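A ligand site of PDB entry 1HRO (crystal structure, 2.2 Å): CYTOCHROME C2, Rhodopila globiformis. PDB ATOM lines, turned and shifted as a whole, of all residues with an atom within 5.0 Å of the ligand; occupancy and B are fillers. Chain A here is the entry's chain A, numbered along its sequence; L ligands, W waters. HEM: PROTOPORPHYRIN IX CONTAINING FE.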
ATOM      1  N   ILE A  18       2.400  -6.756 -19.167  1.00  0.00           N
ATOM      2  CA  ILE A  18       2.091  -6.499 -17.788  1.00  0.00           C
ATOM      3  C   ILE A  18       0.638  -6.199 -17.531  1.00  0.00           C
ATOM      4  O   ILE A  18      -0.058  -6.946 -16.854  1.00  0.00           O
ATOM      5  CB  ILE A  18       2.937  -5.288 -17.339  1.00  0.00           C
ATOM      6  CG1 ILE A  18       4.421  -5.444 -17.646  1.00  0.00           C
ATOM      7  CG2 ILE A  18       2.828  -5.016 -15.857  1.00  0.00           C
ATOM      8  CD1 ILE A  18       5.227  -4.223 -17.263  1.00  0.00           C
ATOM      9  N   CYS A  19       0.206  -5.045 -18.044  1.00  0.00           N
ATOM     10  CA  CYS A  19      -1.163  -4.540 -17.831  1.00  0.00           C
ATOM     11  C   CYS A  19      -2.251  -5.451 -18.384  1.00  0.00           C
ATOM     12  O   CYS A  19      -3.355  -5.585 -17.810  1.00  0.00           O
ATOM     13  CB  CYS A  19      -1.332  -3.107 -18.450  1.00  0.00           C
ATOM     14  SG  CYS A  19      -0.106  -1.928 -17.825  1.00  0.00           S
ATOM     15  N   THR A  21      -2.595  -8.412 -18.508  1.00  0.00           N
ATOM     16  CA  THR A  21      -2.924  -9.563 -17.672  1.00  0.00           C
ATOM     17  C   THR A  21      -4.260  -9.345 -16.956  1.00  0.00           C
ATOM     18  O   THR A  21      -4.977 -10.280 -16.611  1.00  0.00           O
ATOM     19  CB  THR A  21      -1.796  -9.827 -16.648  1.00  0.00           C
ATOM     20  OG1 THR A  21      -0.618 -10.287 -17.321  1.00  0.00           O
ATOM     21  CG2 THR A  21      -2.166 -10.885 -15.590  1.00  0.00           C
ATOM     22  N   CYS A  22      -4.588  -8.063 -16.718  1.00  0.00           N
ATOM     23  CA  CYS A  22      -5.815  -7.676 -16.009  1.00  0.00           C
ATOM     24  C   CYS A  22      -6.680  -6.677 -16.773  1.00  0.00           C
ATOM     25  O   CYS A  22      -7.911  -6.556 -16.587  1.00  0.00           O
ATOM     26  CB  CYS A  22      -5.519  -7.034 -14.661  1.00  0.00           C
ATOM     27  SG  CYS A  22      -4.785  -8.229 -13.492  1.00  0.00           S
ATOM     28  N   HIS A  23      -6.051  -5.934 -17.688  1.00  0.00           N
ATOM     29  CA  HIS A  23      -6.733  -4.920 -18.517  1.00  0.00           C
ATOM     30  C   HIS A  23      -6.606  -5.162 -20.031  1.00  0.00           C
ATOM     31  O   HIS A  23      -5.837  -6.021 -20.518  1.00  0.00           O
ATOM     32  CB  HIS A  23      -6.117  -3.525 -18.308  1.00  0.00           C
ATOM     33  CG  HIS A  23      -6.109  -3.053 -16.861  1.00  0.00           C
ATOM     34  ND1 HIS A  23      -7.231  -2.465 -16.267  1.00  0.00           N
ATOM     35  CD2 HIS A  23      -5.144  -3.066 -15.930  1.00  0.00           C
ATOM     36  CE1 HIS A  23      -6.920  -2.171 -15.023  1.00  0.00           C
ATOM     37  NE2 HIS A  23      -5.667  -2.532 -14.786  1.00  0.00           N
ATOM     38  N   VAL A  32     -10.722  -8.230 -15.691  1.00  0.00           N
ATOM     39  CA  VAL A  32     -10.545  -8.215 -14.238  1.00  0.00           C
ATOM     40  C   VAL A  32     -10.534  -6.766 -13.831  1.00  0.00           C
ATOM     41  O   VAL A  32     -11.005  -6.380 -12.756  1.00  0.00           O
ATOM     42  CB  VAL A  32      -9.250  -8.941 -13.860  1.00  0.00           C
ATOM     43  CG1 VAL A  32      -8.662  -8.555 -12.498  1.00  0.00           C
ATOM     44  CG2 VAL A  32      -9.384 -10.454 -14.061  1.00  0.00           C
ATOM     45  N   GLY A  33      -9.940  -5.966 -14.724  1.00  0.00           N
ATOM     46  CA  GLY A  33      -9.820  -4.512 -14.592  1.00  0.00           C
ATOM     47  C   GLY A  33     -10.620  -3.820 -15.744  1.00  0.00           C
ATOM     48  O   GLY A  33     -10.957  -4.464 -16.774  1.00  0.00           O
ATOM     49  N   PRO A  34     -10.923  -2.506 -15.620  1.00  0.00           N
ATOM     50  CA  PRO A  34     -11.682  -1.790 -16.644  1.00  0.00           C
ATOM     51  C   PRO A  34     -10.824  -1.483 -17.885  1.00  0.00           C
ATOM     52  O   PRO A  34      -9.616  -1.448 -17.817  1.00  0.00           O
ATOM     53  CB  PRO A  34     -12.144  -0.457 -15.983  1.00  0.00           C
ATOM     54  CG  PRO A  34     -11.197  -0.260 -14.782  1.00  0.00           C
ATOM     55  CD  PRO A  34     -10.620  -1.605 -14.446  1.00  0.00           C
ATOM     56  N   LEU A  36      -8.524   0.224 -20.381  1.00  0.00           N
ATOM     57  CA  LEU A  36      -7.630   1.378 -20.256  1.00  0.00           C
ATOM     58  C   LEU A  36      -7.682   2.304 -21.498  1.00  0.00           C
ATOM     59  O   LEU A  36      -6.962   3.313 -21.596  1.00  0.00           O
ATOM     60  CB  LEU A  36      -6.222   0.983 -19.857  1.00  0.00           C
ATOM     61  CG  LEU A  36      -6.187   0.386 -18.442  1.00  0.00           C
ATOM     62  CD1 LEU A  36      -4.744   0.201 -17.967  1.00  0.00           C
ATOM     63  CD2 LEU A  36      -6.940   1.262 -17.473  1.00  0.00           C
ATOM     64  N   VAL A  39      -8.190   6.104 -21.091  1.00  0.00           N
ATOM     65  CA  VAL A  39      -8.063   6.372 -19.649  1.00  0.00           C
ATOM     66  C   VAL A  39      -7.468   7.747 -19.241  1.00  0.00           C
ATOM     67  O   VAL A  39      -7.752   8.299 -18.140  1.00  0.00           O
ATOM     68  CB  VAL A  39      -7.401   5.205 -18.895  1.00  0.00           C
ATOM     69  CG1 VAL A  39      -5.917   5.105 -19.289  1.00  0.00           C
ATOM     70  CG2 VAL A  39      -7.540   5.421 -17.389  1.00  0.00           C
ATOM     71  N   ARG A  42      -9.446  10.667 -18.069  1.00  0.00           N
ATOM     72  CA  ARG A  42     -10.736  10.212 -17.599  1.00  0.00           C
ATOM     73  C   ARG A  42     -10.787  10.295 -16.072  1.00  0.00           C
ATOM     74  O   ARG A  42      -9.759  10.174 -15.347  1.00  0.00           O
ATOM     75  CB  ARG A  42     -10.825   8.732 -17.975  1.00  0.00           C
ATOM     76  CG  ARG A  42     -12.175   8.006 -17.866  1.00  0.00           C
ATOM     77  CD  ARG A  42     -12.188   6.685 -18.652  1.00  0.00           C
ATOM     78  NE  ARG A  42     -11.901   5.443 -17.869  1.00  0.00           N
ATOM     79  CZ  ARG A  42     -11.389   4.282 -18.401  1.00  0.00           C
ATOM     80  NH1 ARG A  42     -11.028   4.115 -19.676  1.00  0.00           N
ATOM     81  NH2 ARG A  42     -11.184   3.237 -17.628  1.00  0.00           N
ATOM     82  N   HIS A  43     -12.011  10.469 -15.594  1.00  0.00           N
ATOM     83  CA  HIS A  43     -12.276  10.487 -14.176  1.00  0.00           C
ATOM     84  C   HIS A  43     -12.327   9.024 -13.730  1.00  0.00           C
ATOM     85  O   HIS A  43     -12.874   8.206 -14.479  1.00  0.00           O
ATOM     86  CB  HIS A  43     -13.704  11.004 -13.959  1.00  0.00           C
ATOM     87  CG  HIS A  43     -13.928  11.521 -12.585  1.00  0.00           C
ATOM     88  ND1 HIS A  43     -14.236  10.689 -11.533  1.00  0.00           N
ATOM     89  CD2 HIS A  43     -13.849  12.771 -12.130  1.00  0.00           C
ATOM     90  CE1 HIS A  43     -14.352  11.465 -10.467  1.00  0.00           C
ATOM     91  NE2 HIS A  43     -14.121  12.702 -10.791  1.00  0.00           N
ATOM     92  N   SER A  44     -11.832   8.734 -12.529  1.00  0.00           N
ATOM     93  CA  SER A  44     -11.886   7.390 -12.008  1.00  0.00           C
ATOM     94  C   SER A  44     -13.349   6.917 -11.864  1.00  0.00           C
ATOM     95  O   SER A  44     -14.263   7.731 -11.774  1.00  0.00           O
ATOM     96  CB  SER A  44     -11.177   7.289 -10.673  1.00  0.00           C
ATOM     97  OG  SER A  44     -11.592   8.328  -9.864  1.00  0.00           O
ATOM     98  N   GLY A  45     -13.519   5.582 -11.833  1.00  0.00           N
ATOM     99  CA  GLY A  45     -14.779   4.875 -11.670  1.00  0.00           C
ATOM    100  C   GLY A  45     -15.907   5.140 -12.694  1.00  0.00           C
ATOM    101  O   GLY A  45     -17.095   5.002 -12.401  1.00  0.00           O
ATOM    102  N   ILE A  46     -15.585   5.456 -13.933  1.00  0.00           N
ATOM    103  CA  ILE A  46     -16.681   5.727 -14.817  1.00  0.00           C
ATOM    104  C   ILE A  46     -16.872   4.772 -15.972  1.00  0.00           C
ATOM    105  O   ILE A  46     -17.818   4.869 -16.745  1.00  0.00           O
ATOM    106  CB  ILE A  46     -16.733   7.192 -15.211  1.00  0.00           C
ATOM    107  CG1 ILE A  46     -15.591   7.488 -16.188  1.00  0.00           C
ATOM    108  CG2 ILE A  46     -16.650   8.067 -13.947  1.00  0.00           C
ATOM    109  CD1 ILE A  46     -15.821   8.691 -17.110  1.00  0.00           C
ATOM    110  N   TYR A  50     -18.350  -1.658 -15.516  1.00  0.00           N
ATOM    111  CA  TYR A  50     -17.264  -2.223 -14.714  1.00  0.00           C
ATOM    112  C   TYR A  50     -17.555  -2.157 -13.226  1.00  0.00           C
ATOM    113  O   TYR A  50     -18.051  -1.167 -12.720  1.00  0.00           O
ATOM    114  CB  TYR A  50     -15.888  -1.589 -15.020  1.00  0.00           C
ATOM    115  CG  TYR A  50     -14.888  -2.182 -14.118  1.00  0.00           C
ATOM    116  CD1 TYR A  50     -14.311  -3.395 -14.473  1.00  0.00           C
ATOM    117  CD2 TYR A  50     -14.592  -1.615 -12.868  1.00  0.00           C
ATOM    118  CE1 TYR A  50     -13.427  -4.061 -13.638  1.00  0.00           C
ATOM    119  CE2 TYR A  50     -13.702  -2.253 -12.003  1.00  0.00           C
ATOM    120  CZ  TYR A  50     -13.133  -3.463 -12.415  1.00  0.00           C
ATOM    121  OH  TYR A  50     -12.262  -4.079 -11.615  1.00  0.00           O
ATOM    122  N   ASN A  51     -17.239  -3.218 -12.510  1.00  0.00           N
ATOM    123  CA  ASN A  51     -17.503  -3.226 -11.079  1.00  0.00           C
ATOM    124  C   ASN A  51     -16.321  -2.706 -10.243  1.00  0.00           C
ATOM    125  O   ASN A  51     -15.492  -3.465  -9.795  1.00  0.00           O
ATOM    126  CB  ASN A  51     -17.906  -4.651 -10.692  1.00  0.00           C
ATOM    127  CG  ASN A  51     -18.082  -4.837  -9.216  1.00  0.00           C
ATOM    128  OD1 ASN A  51     -17.625  -5.843  -8.660  1.00  0.00           O
ATOM    129  ND2 ASN A  51     -18.778  -3.902  -8.610  1.00  0.00           N
ATOM    130  N   TYR A  52     -16.244  -1.415 -10.073  1.00  0.00           N
ATOM    131  CA  TYR A  52     -15.230  -0.697  -9.346  1.00  0.00           C
ATOM    132  C   TYR A  52     -15.379  -0.930  -7.874  1.00  0.00           C
ATOM    133  O   TYR A  52     -16.418  -1.329  -7.377  1.00  0.00           O
ATOM    134  CB  TYR A  52     -15.337   0.870  -9.543  1.00  0.00           C
ATOM    135  CG  TYR A  52     -14.873   1.363 -10.903  1.00  0.00           C
ATOM    136  CD1 TYR A  52     -13.531   1.642 -11.173  1.00  0.00           C
ATOM    137  CD2 TYR A  52     -15.768   1.526 -11.962  1.00  0.00           C
ATOM    138  CE1 TYR A  52     -13.118   2.046 -12.442  1.00  0.00           C
ATOM    139  CE2 TYR A  52     -15.385   1.949 -13.235  1.00  0.00           C
ATOM    140  CZ  TYR A  52     -14.029   2.232 -13.476  1.00  0.00           C
ATOM    141  OH  TYR A  52     -13.592   2.649 -14.721  1.00  0.00           O
ATOM    142  N   SER A  53     -14.314  -0.659  -7.181  1.00  0.00           N
ATOM    143  CA  SER A  53     -14.298  -0.739  -5.751  1.00  0.00           C
ATOM    144  C   SER A  53     -14.831   0.575  -5.207  1.00  0.00           C
ATOM    145  O   SER A  53     -14.954   1.605  -5.906  1.00  0.00           O
ATOM    146  CB  SER A  53     -12.909  -1.026  -5.189  1.00  0.00           C
ATOM    147  OG  SER A  53     -12.159   0.167  -5.218  1.00  0.00           O
ATOM    148  N   ASN A  56     -12.050   3.335  -5.310  1.00  0.00           N
ATOM    149  CA  ASN A  56     -11.890   3.984  -6.594  1.00  0.00           C
ATOM    150  C   ASN A  56     -12.997   4.981  -6.899  1.00  0.00           C
ATOM    151  O   ASN A  56     -12.790   6.094  -7.394  1.00  0.00           O
ATOM    152  CB  ASN A  56     -11.769   2.915  -7.723  1.00  0.00           C
ATOM    153  CG  ASN A  56     -11.695   3.566  -9.106  1.00  0.00           C
ATOM    154  OD1 ASN A  56     -12.616   4.263  -9.538  1.00  0.00           O
ATOM    155  ND2 ASN A  56     -10.589   3.343  -9.800  1.00  0.00           N
ATOM    156  N   TRP A  63      -7.565  10.791 -14.038  1.00  0.00           N
ATOM    157  CA  TRP A  63      -6.353  10.184 -14.500  1.00  0.00           C
ATOM    158  C   TRP A  63      -5.420  10.994 -15.369  1.00  0.00           C
ATOM    159  O   TRP A  63      -5.231  10.705 -16.525  1.00  0.00           O
ATOM    160  CB  TRP A  63      -6.753   8.821 -15.088  1.00  0.00           C
ATOM    161  CG  TRP A  63      -7.265   7.883 -14.010  1.00  0.00           C
ATOM    162  CD1 TRP A  63      -8.488   7.300 -13.979  1.00  0.00           C
ATOM    163  CD2 TRP A  63      -6.567   7.443 -12.825  1.00  0.00           C
ATOM    164  NE1 TRP A  63      -8.590   6.509 -12.859  1.00  0.00           N
ATOM    165  CE2 TRP A  63      -7.443   6.566 -12.148  1.00  0.00           C
ATOM    166  CE3 TRP A  63      -5.283   7.621 -12.319  1.00  0.00           C
ATOM    167  CZ2 TRP A  63      -7.076   5.900 -10.988  1.00  0.00           C
ATOM    168  CZ3 TRP A  63      -4.916   6.964 -11.163  1.00  0.00           C
ATOM    169  CH2 TRP A  63      -5.801   6.119 -10.490  1.00  0.00           C
ATOM    170  N   LEU A  68      -1.277   9.238 -12.935  1.00  0.00           N
ATOM    171  CA  LEU A  68      -1.029   7.895 -13.412  1.00  0.00           C
ATOM    172  C   LEU A  68       0.440   7.530 -13.087  1.00  0.00           C
ATOM    173  O   LEU A  68       0.754   6.419 -12.701  1.00  0.00           O
ATOM    174  CB  LEU A  68      -1.262   7.813 -14.945  1.00  0.00           C
ATOM    175  CG  LEU A  68      -2.682   7.583 -15.456  1.00  0.00           C
ATOM    176  CD1 LEU A  68      -2.802   7.833 -16.968  1.00  0.00           C
ATOM    177  CD2 LEU A  68      -3.188   6.180 -15.152  1.00  0.00           C
ATOM    178  N   TYR A  71       0.526   6.585  -9.336  1.00  0.00           N
ATOM    179  CA  TYR A  71      -0.337   5.443  -9.141  1.00  0.00           C
ATOM    180  C   TYR A  71       0.279   4.148  -9.609  1.00  0.00           C
ATOM    181  O   TYR A  71       0.219   3.132  -8.917  1.00  0.00           O
ATOM    182  CB  TYR A  71      -1.677   5.717  -9.901  1.00  0.00           C
ATOM    183  CG  TYR A  71      -2.618   4.542  -9.869  1.00  0.00           C
ATOM    184  CD1 TYR A  71      -3.257   4.269  -8.663  1.00  0.00           C
ATOM    185  CD2 TYR A  71      -2.867   3.739 -10.991  1.00  0.00           C
ATOM    186  CE1 TYR A  71      -4.119   3.187  -8.546  1.00  0.00           C
ATOM    187  CE2 TYR A  71      -3.714   2.624 -10.894  1.00  0.00           C
ATOM    188  CZ  TYR A  71      -4.328   2.363  -9.665  1.00  0.00           C
ATOM    189  OH  TYR A  71      -5.167   1.338  -9.548  1.00  0.00           O
ATOM    190  N   ILE A  72       0.829   4.153 -10.827  1.00  0.00           N
ATOM    191  CA  ILE A  72       1.444   2.958 -11.405  1.00  0.00           C
ATOM    192  C   ILE A  72       2.627   2.449 -10.525  1.00  0.00           C
ATOM    193  O   ILE A  72       2.942   1.254 -10.427  1.00  0.00           O
ATOM    194  CB  ILE A  72       1.838   3.192 -12.866  1.00  0.00           C
ATOM    195  CG1 ILE A  72       0.602   3.311 -13.689  1.00  0.00           C
ATOM    196  CG2 ILE A  72       2.599   2.013 -13.423  1.00  0.00           C
ATOM    197  CD1 ILE A  72       0.978   3.533 -15.129  1.00  0.00           C
ATOM    198  N   THR A  82      -7.757   0.140  -3.100  1.00  0.00           N
ATOM    199  CA  THR A  82      -8.090  -0.294  -4.438  1.00  0.00           C
ATOM    200  C   THR A  82      -7.972  -1.773  -4.589  1.00  0.00           C
ATOM    201  O   THR A  82      -7.245  -2.412  -3.865  1.00  0.00           O
ATOM    202  CB  THR A  82      -7.332   0.464  -5.568  1.00  0.00           C
ATOM    203  OG1 THR A  82      -7.709   0.021  -6.858  1.00  0.00           O
ATOM    204  CG2 THR A  82      -5.844   0.277  -5.445  1.00  0.00           C
ATOM    205  N   LYS A  83      -8.698  -2.340  -5.473  1.00  0.00           N
ATOM    206  CA  LYS A  83      -8.584  -3.747  -5.615  1.00  0.00           C
ATOM    207  C   LYS A  83      -7.570  -4.113  -6.722  1.00  0.00           C
ATOM    208  O   LYS A  83      -7.426  -5.281  -7.077  1.00  0.00           O
ATOM    209  CB  LYS A  83      -9.947  -4.441  -5.659  1.00  0.00           C
ATOM    210  CG  LYS A  83     -10.717  -4.239  -6.968  1.00  0.00           C
ATOM    211  CD  LYS A  83     -11.964  -5.119  -7.049  1.00  0.00           C
ATOM    212  CE  LYS A  83     -13.109  -4.482  -7.797  1.00  0.00           C
ATOM    213  NZ  LYS A  83     -14.216  -5.443  -7.930  1.00  0.00           N
ATOM    214  N   MET A  84      -6.869  -3.139  -7.314  1.00  0.00           N
ATOM    215  CA  MET A  84      -5.841  -3.445  -8.351  1.00  0.00           C
ATOM    216  C   MET A  84      -4.604  -4.001  -7.628  1.00  0.00           C
ATOM    217  O   MET A  84      -3.898  -3.265  -6.934  1.00  0.00           O
ATOM    218  CB  MET A  84      -5.422  -2.179  -9.104  1.00  0.00           C
ATOM    219  CG  MET A  84      -4.073  -2.245  -9.789  1.00  0.00           C
ATOM    220  SD  MET A  84      -4.064  -1.071 -11.187  1.00  0.00           S
ATOM    221  CE  MET A  84      -2.283  -0.744 -11.324  1.00  0.00           C
ATOM    222  N   GLY A  85      -4.378  -5.308  -7.799  1.00  0.00           N
ATOM    223  CA  GLY A  85      -3.325  -6.154  -7.185  1.00  0.00           C
ATOM    224  C   GLY A  85      -1.845  -5.967  -7.571  1.00  0.00           C
ATOM    225  O   GLY A  85      -0.962  -6.521  -6.910  1.00  0.00           O
ATOM    226  N   TYR A  86      -1.580  -5.199  -8.615  1.00  0.00           N
ATOM    227  CA  TYR A  86      -0.260  -4.899  -9.100  1.00  0.00           C
ATOM    228  C   TYR A  86       0.622  -4.258  -8.020  1.00  0.00           C
ATOM    229  O   TYR A  86       0.281  -3.172  -7.595  1.00  0.00           O
ATOM    230  CB  TYR A  86      -0.386  -3.938 -10.314  1.00  0.00           C
ATOM    231  CG  TYR A  86       0.920  -3.716 -11.053  1.00  0.00           C
ATOM    232  CD1 TYR A  86       1.705  -4.769 -11.566  1.00  0.00           C
ATOM    233  CD2 TYR A  86       1.388  -2.418 -11.235  1.00  0.00           C
ATOM    234  CE1 TYR A  86       2.884  -4.553 -12.267  1.00  0.00           C
ATOM    235  CE2 TYR A  86       2.608  -2.185 -11.883  1.00  0.00           C
ATOM    236  CZ  TYR A  86       3.351  -3.241 -12.399  1.00  0.00           C
ATOM    237  OH  TYR A  86       4.552  -3.052 -13.089  1.00  0.00           O
ATOM    238  N   ILE A  98       4.884   3.495 -20.368  1.00  0.00           N
ATOM    239  CA  ILE A  98       3.527   3.018 -20.322  1.00  0.00           C
ATOM    240  C   ILE A  98       2.567   4.178 -20.454  1.00  0.00           C
ATOM    241  O   ILE A  98       1.609   4.089 -21.171  1.00  0.00           O
ATOM    242  CB  ILE A  98       3.203   2.169 -19.108  1.00  0.00           C
ATOM    243  CG1 ILE A  98       3.994   0.868 -19.168  1.00  0.00           C
ATOM    244  CG2 ILE A  98       1.698   1.930 -18.989  1.00  0.00           C
ATOM    245  CD1 ILE A  98       4.238   0.273 -17.782  1.00  0.00           C
ATOM    246  N   LEU A 102      -0.514   4.931 -23.192  1.00  0.00           N
ATOM    247  CA  LEU A 102      -1.882   5.178 -22.761  1.00  0.00           C
ATOM    248  C   LEU A 102      -2.429   6.358 -23.497  1.00  0.00           C
ATOM    249  O   LEU A 102      -3.609   6.440 -23.817  1.00  0.00           O
ATOM    250  CB  LEU A 102      -1.902   5.430 -21.215  1.00  0.00           C
ATOM    251  CG  LEU A 102      -1.669   4.119 -20.432  1.00  0.00           C
ATOM    252  CD1 LEU A 102      -1.821   4.375 -18.955  1.00  0.00           C
ATOM    253  CD2 LEU A 102      -2.706   3.081 -20.800  1.00  0.00           C
HETATM  254  CHA HEM L   1      -7.731  -0.202 -12.134  1.00  0.00           C
HETATM  255  CHB HEM L   1      -3.872   1.060 -14.612  1.00  0.00           C
HETATM  256  CHC HEM L   1      -2.110  -3.366 -14.171  1.00  0.00           C
HETATM  257  CHD HEM L   1      -6.201  -4.725 -11.908  1.00  0.00           C
HETATM  258  C1A HEM L   1      -6.832   0.582 -12.753  1.00  0.00           C
HETATM  259  C2A HEM L   1      -6.952   1.995 -13.049  1.00  0.00           C
HETATM  260  C3A HEM L   1      -5.859   2.345 -13.771  1.00  0.00           C
HETATM  261  C4A HEM L   1      -5.064   1.181 -13.916  1.00  0.00           C
HETATM  262  CMA HEM L   1      -5.490   3.740 -14.297  1.00  0.00           C
HETATM  263  CAA HEM L   1      -8.132   2.867 -12.665  1.00  0.00           C
HETATM  264  CBA HEM L   1      -9.011   3.189 -13.938  1.00  0.00           C
HETATM  265  CGA HEM L   1     -10.400   3.778 -13.628  1.00  0.00           C
HETATM  266  O1A HEM L   1     -11.252   3.542 -14.459  1.00  0.00           O
HETATM  267  O2A HEM L   1     -10.629   4.414 -12.650  1.00  0.00           O
HETATM  268  C1B HEM L   1      -3.114  -0.057 -14.753  1.00  0.00           C
HETATM  269  C2B HEM L   1      -1.891  -0.101 -15.541  1.00  0.00           C
HETATM  270  C3B HEM L   1      -1.432  -1.317 -15.425  1.00  0.00           C
HETATM  271  C4B HEM L   1      -2.296  -2.065 -14.590  1.00  0.00           C
HETATM  272  CMB HEM L   1      -1.365   1.057 -16.418  1.00  0.00           C
HETATM  273  CAB HEM L   1      -0.184  -1.880 -15.998  1.00  0.00           C
HETATM  274  CBB HEM L   1       1.192  -1.518 -15.619  1.00  0.00           C
HETATM  275  C1C HEM L   1      -3.082  -4.060 -13.529  1.00  0.00           C
HETATM  276  C2C HEM L   1      -2.965  -5.473 -13.255  1.00  0.00           C
HETATM  277  C3C HEM L   1      -4.129  -5.835 -12.594  1.00  0.00           C
HETATM  278  C4C HEM L   1      -4.971  -4.700 -12.482  1.00  0.00           C
HETATM  279  CMC HEM L   1      -1.785  -6.355 -13.634  1.00  0.00           C
HETATM  280  CAC HEM L   1      -4.479  -7.213 -12.081  1.00  0.00           C
HETATM  281  CBC HEM L   1      -3.574  -8.105 -11.289  1.00  0.00           C
HETATM  282  C1D HEM L   1      -6.964  -3.630 -11.789  1.00  0.00           C
HETATM  283  C2D HEM L   1      -8.283  -3.586 -11.167  1.00  0.00           C
HETATM  284  C3D HEM L   1      -8.714  -2.273 -11.271  1.00  0.00           C
HETATM  285  C4D HEM L   1      -7.662  -1.552 -11.931  1.00  0.00           C
HETATM  286  CMD HEM L   1      -8.968  -4.798 -10.577  1.00  0.00           C
HETATM  287  CAD HEM L   1      -9.953  -1.646 -10.665  1.00  0.00           C
HETATM  288  CBD HEM L   1      -9.646  -1.123  -9.198  1.00  0.00           C
HETATM  289  CGD HEM L   1     -10.763  -0.774  -8.224  1.00  0.00           C
HETATM  290  O1D HEM L   1     -11.937  -0.703  -8.436  1.00  0.00           O
HETATM  291  O2D HEM L   1     -10.396  -0.544  -7.060  1.00  0.00           O
HETATM  292  NA  HEM L   1      -5.644   0.103 -13.291  1.00  0.00           N
HETATM  293  NB  HEM L   1      -3.314  -1.294 -14.171  1.00  0.00           N
HETATM  294  NC  HEM L   1      -4.323  -3.590 -13.068  1.00  0.00           N
HETATM  295  ND  HEM L   1      -6.625  -2.360 -12.208  1.00  0.00           N
HETATM  296 FE   HEM L   1      -4.959  -1.745 -13.120  1.00  0.00          FE
HETATM  297  O   HOH W   1     -12.949   5.606 -15.282  1.00  0.00           O
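The side-chain sulfur of Cys 22 is covalently linked to a carbon (CAC) of the ligand (1.8 Å). SG of Cys 19 is covalently linked to CAB of the ligand, 1.8 Å away. NE2 of His 23 is bound to FE of the ligand, 2.0 Å away. The side-chain sulfur (SD) of Met 84 binds an iron atom (FE) of the ligand (2.2 Å). OH of Tyr 52 sits at hydrogen-bond distance from O1A of the ligand, at 2.5 Å. The backbone NH (N) of Ser 53 sits at hydrogen-bond distance from an oxygen (O1D) of the ligand (2.7 Å). The side-chain hydroxyl of Ser 53 sits at hydrogen-bond distance from an oxygen (O2D) of the ligand, at 2.6 Å. An oxygen (O2D) of the ligand sits at hydrogen-bond distance from the side-chain hydroxyl of Thr 82. The indole nitrogen (NE1) of Trp 63 lies within hydrogen-bond range of an oxygen (O2A) of the ligand, at 2.9 Å. O2D of the ligand sits at hydrogen-bond distance from N of Lys 83 (2.9 Å). The side-chain amide nitrogen of Asn 56 lies within hydrogen-bond range of an oxygen (O2A) of the ligand, 3.0 Å away. An oxygen (O1A) of the ligand is in salt-bridge range of the guanidinium group of Arg 42 (3.2 Å). N of Gly 45 sits at hydrogen-bond distance from O2A of the ligand, 3.2 Å away.
Residues that only touch the ligand: Ser 44 (3.3 Å), Val 32 (3.4 Å), Leu 68 (3.5 Å), Tyr 50 (3.5 Å), Leu 36 (3.6 Å), Tyr 71 (3.6 Å), Ile 72 (3.6 Å), Ile 18 (3.7 Å), Pro 34 (3.8 Å) and Gly 33 (3.9 Å). 22 residues have an atom within 4 Å of the ligand: Ile 18, Cys 19, Cys 22, His 23, Val 32, Gly 33, Pro 34, Leu 36, Arg 42, Ser 44, Gly 45, Tyr 50, Tyr 52, Ser 53, Asn 56, Trp 63, Leu 68, Tyr 71, Ile 72, Thr 82, Lys 83 and Met 84. The nearest printed residue that does not touch the ligand is Tyr 86 (4.1 Å).
The backbone NH (N) of Val 32 lies within hydrogen-bond range of the backbone carbonyl oxygen (O) of Cys 22 (3.4 Å). The side-chain sulfur of Met 84 sits close to the side-chain hydroxyl of Tyr 71 (3.1 Å). The side-chain hydroxyl of Ser 53 lies within hydrogen-bond range of the backbone NH of Asn 56 (3.2 Å). N of Trp 63 lies within hydrogen-bond range of O of Arg 42, 2.6 Å away. The backbone carbonyl oxygen (O) of Asn 51 is in hydrogen-bond range of the side-chain amino group (NZ) of Lys 83 (3.0 Å). The side-chain amide oxygen of Asn 56 sits at hydrogen-bond distance from the backbone NH of Gly 45 (2.8 Å). O of Val 32 lies within hydrogen-bond range of OH of Tyr 50 (2.9 Å). The backbone carbonyl oxygen (O) of Ile 18 lies close to the side-chain hydroxyl (OG1) of Thr 21, 3.4 Å away.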
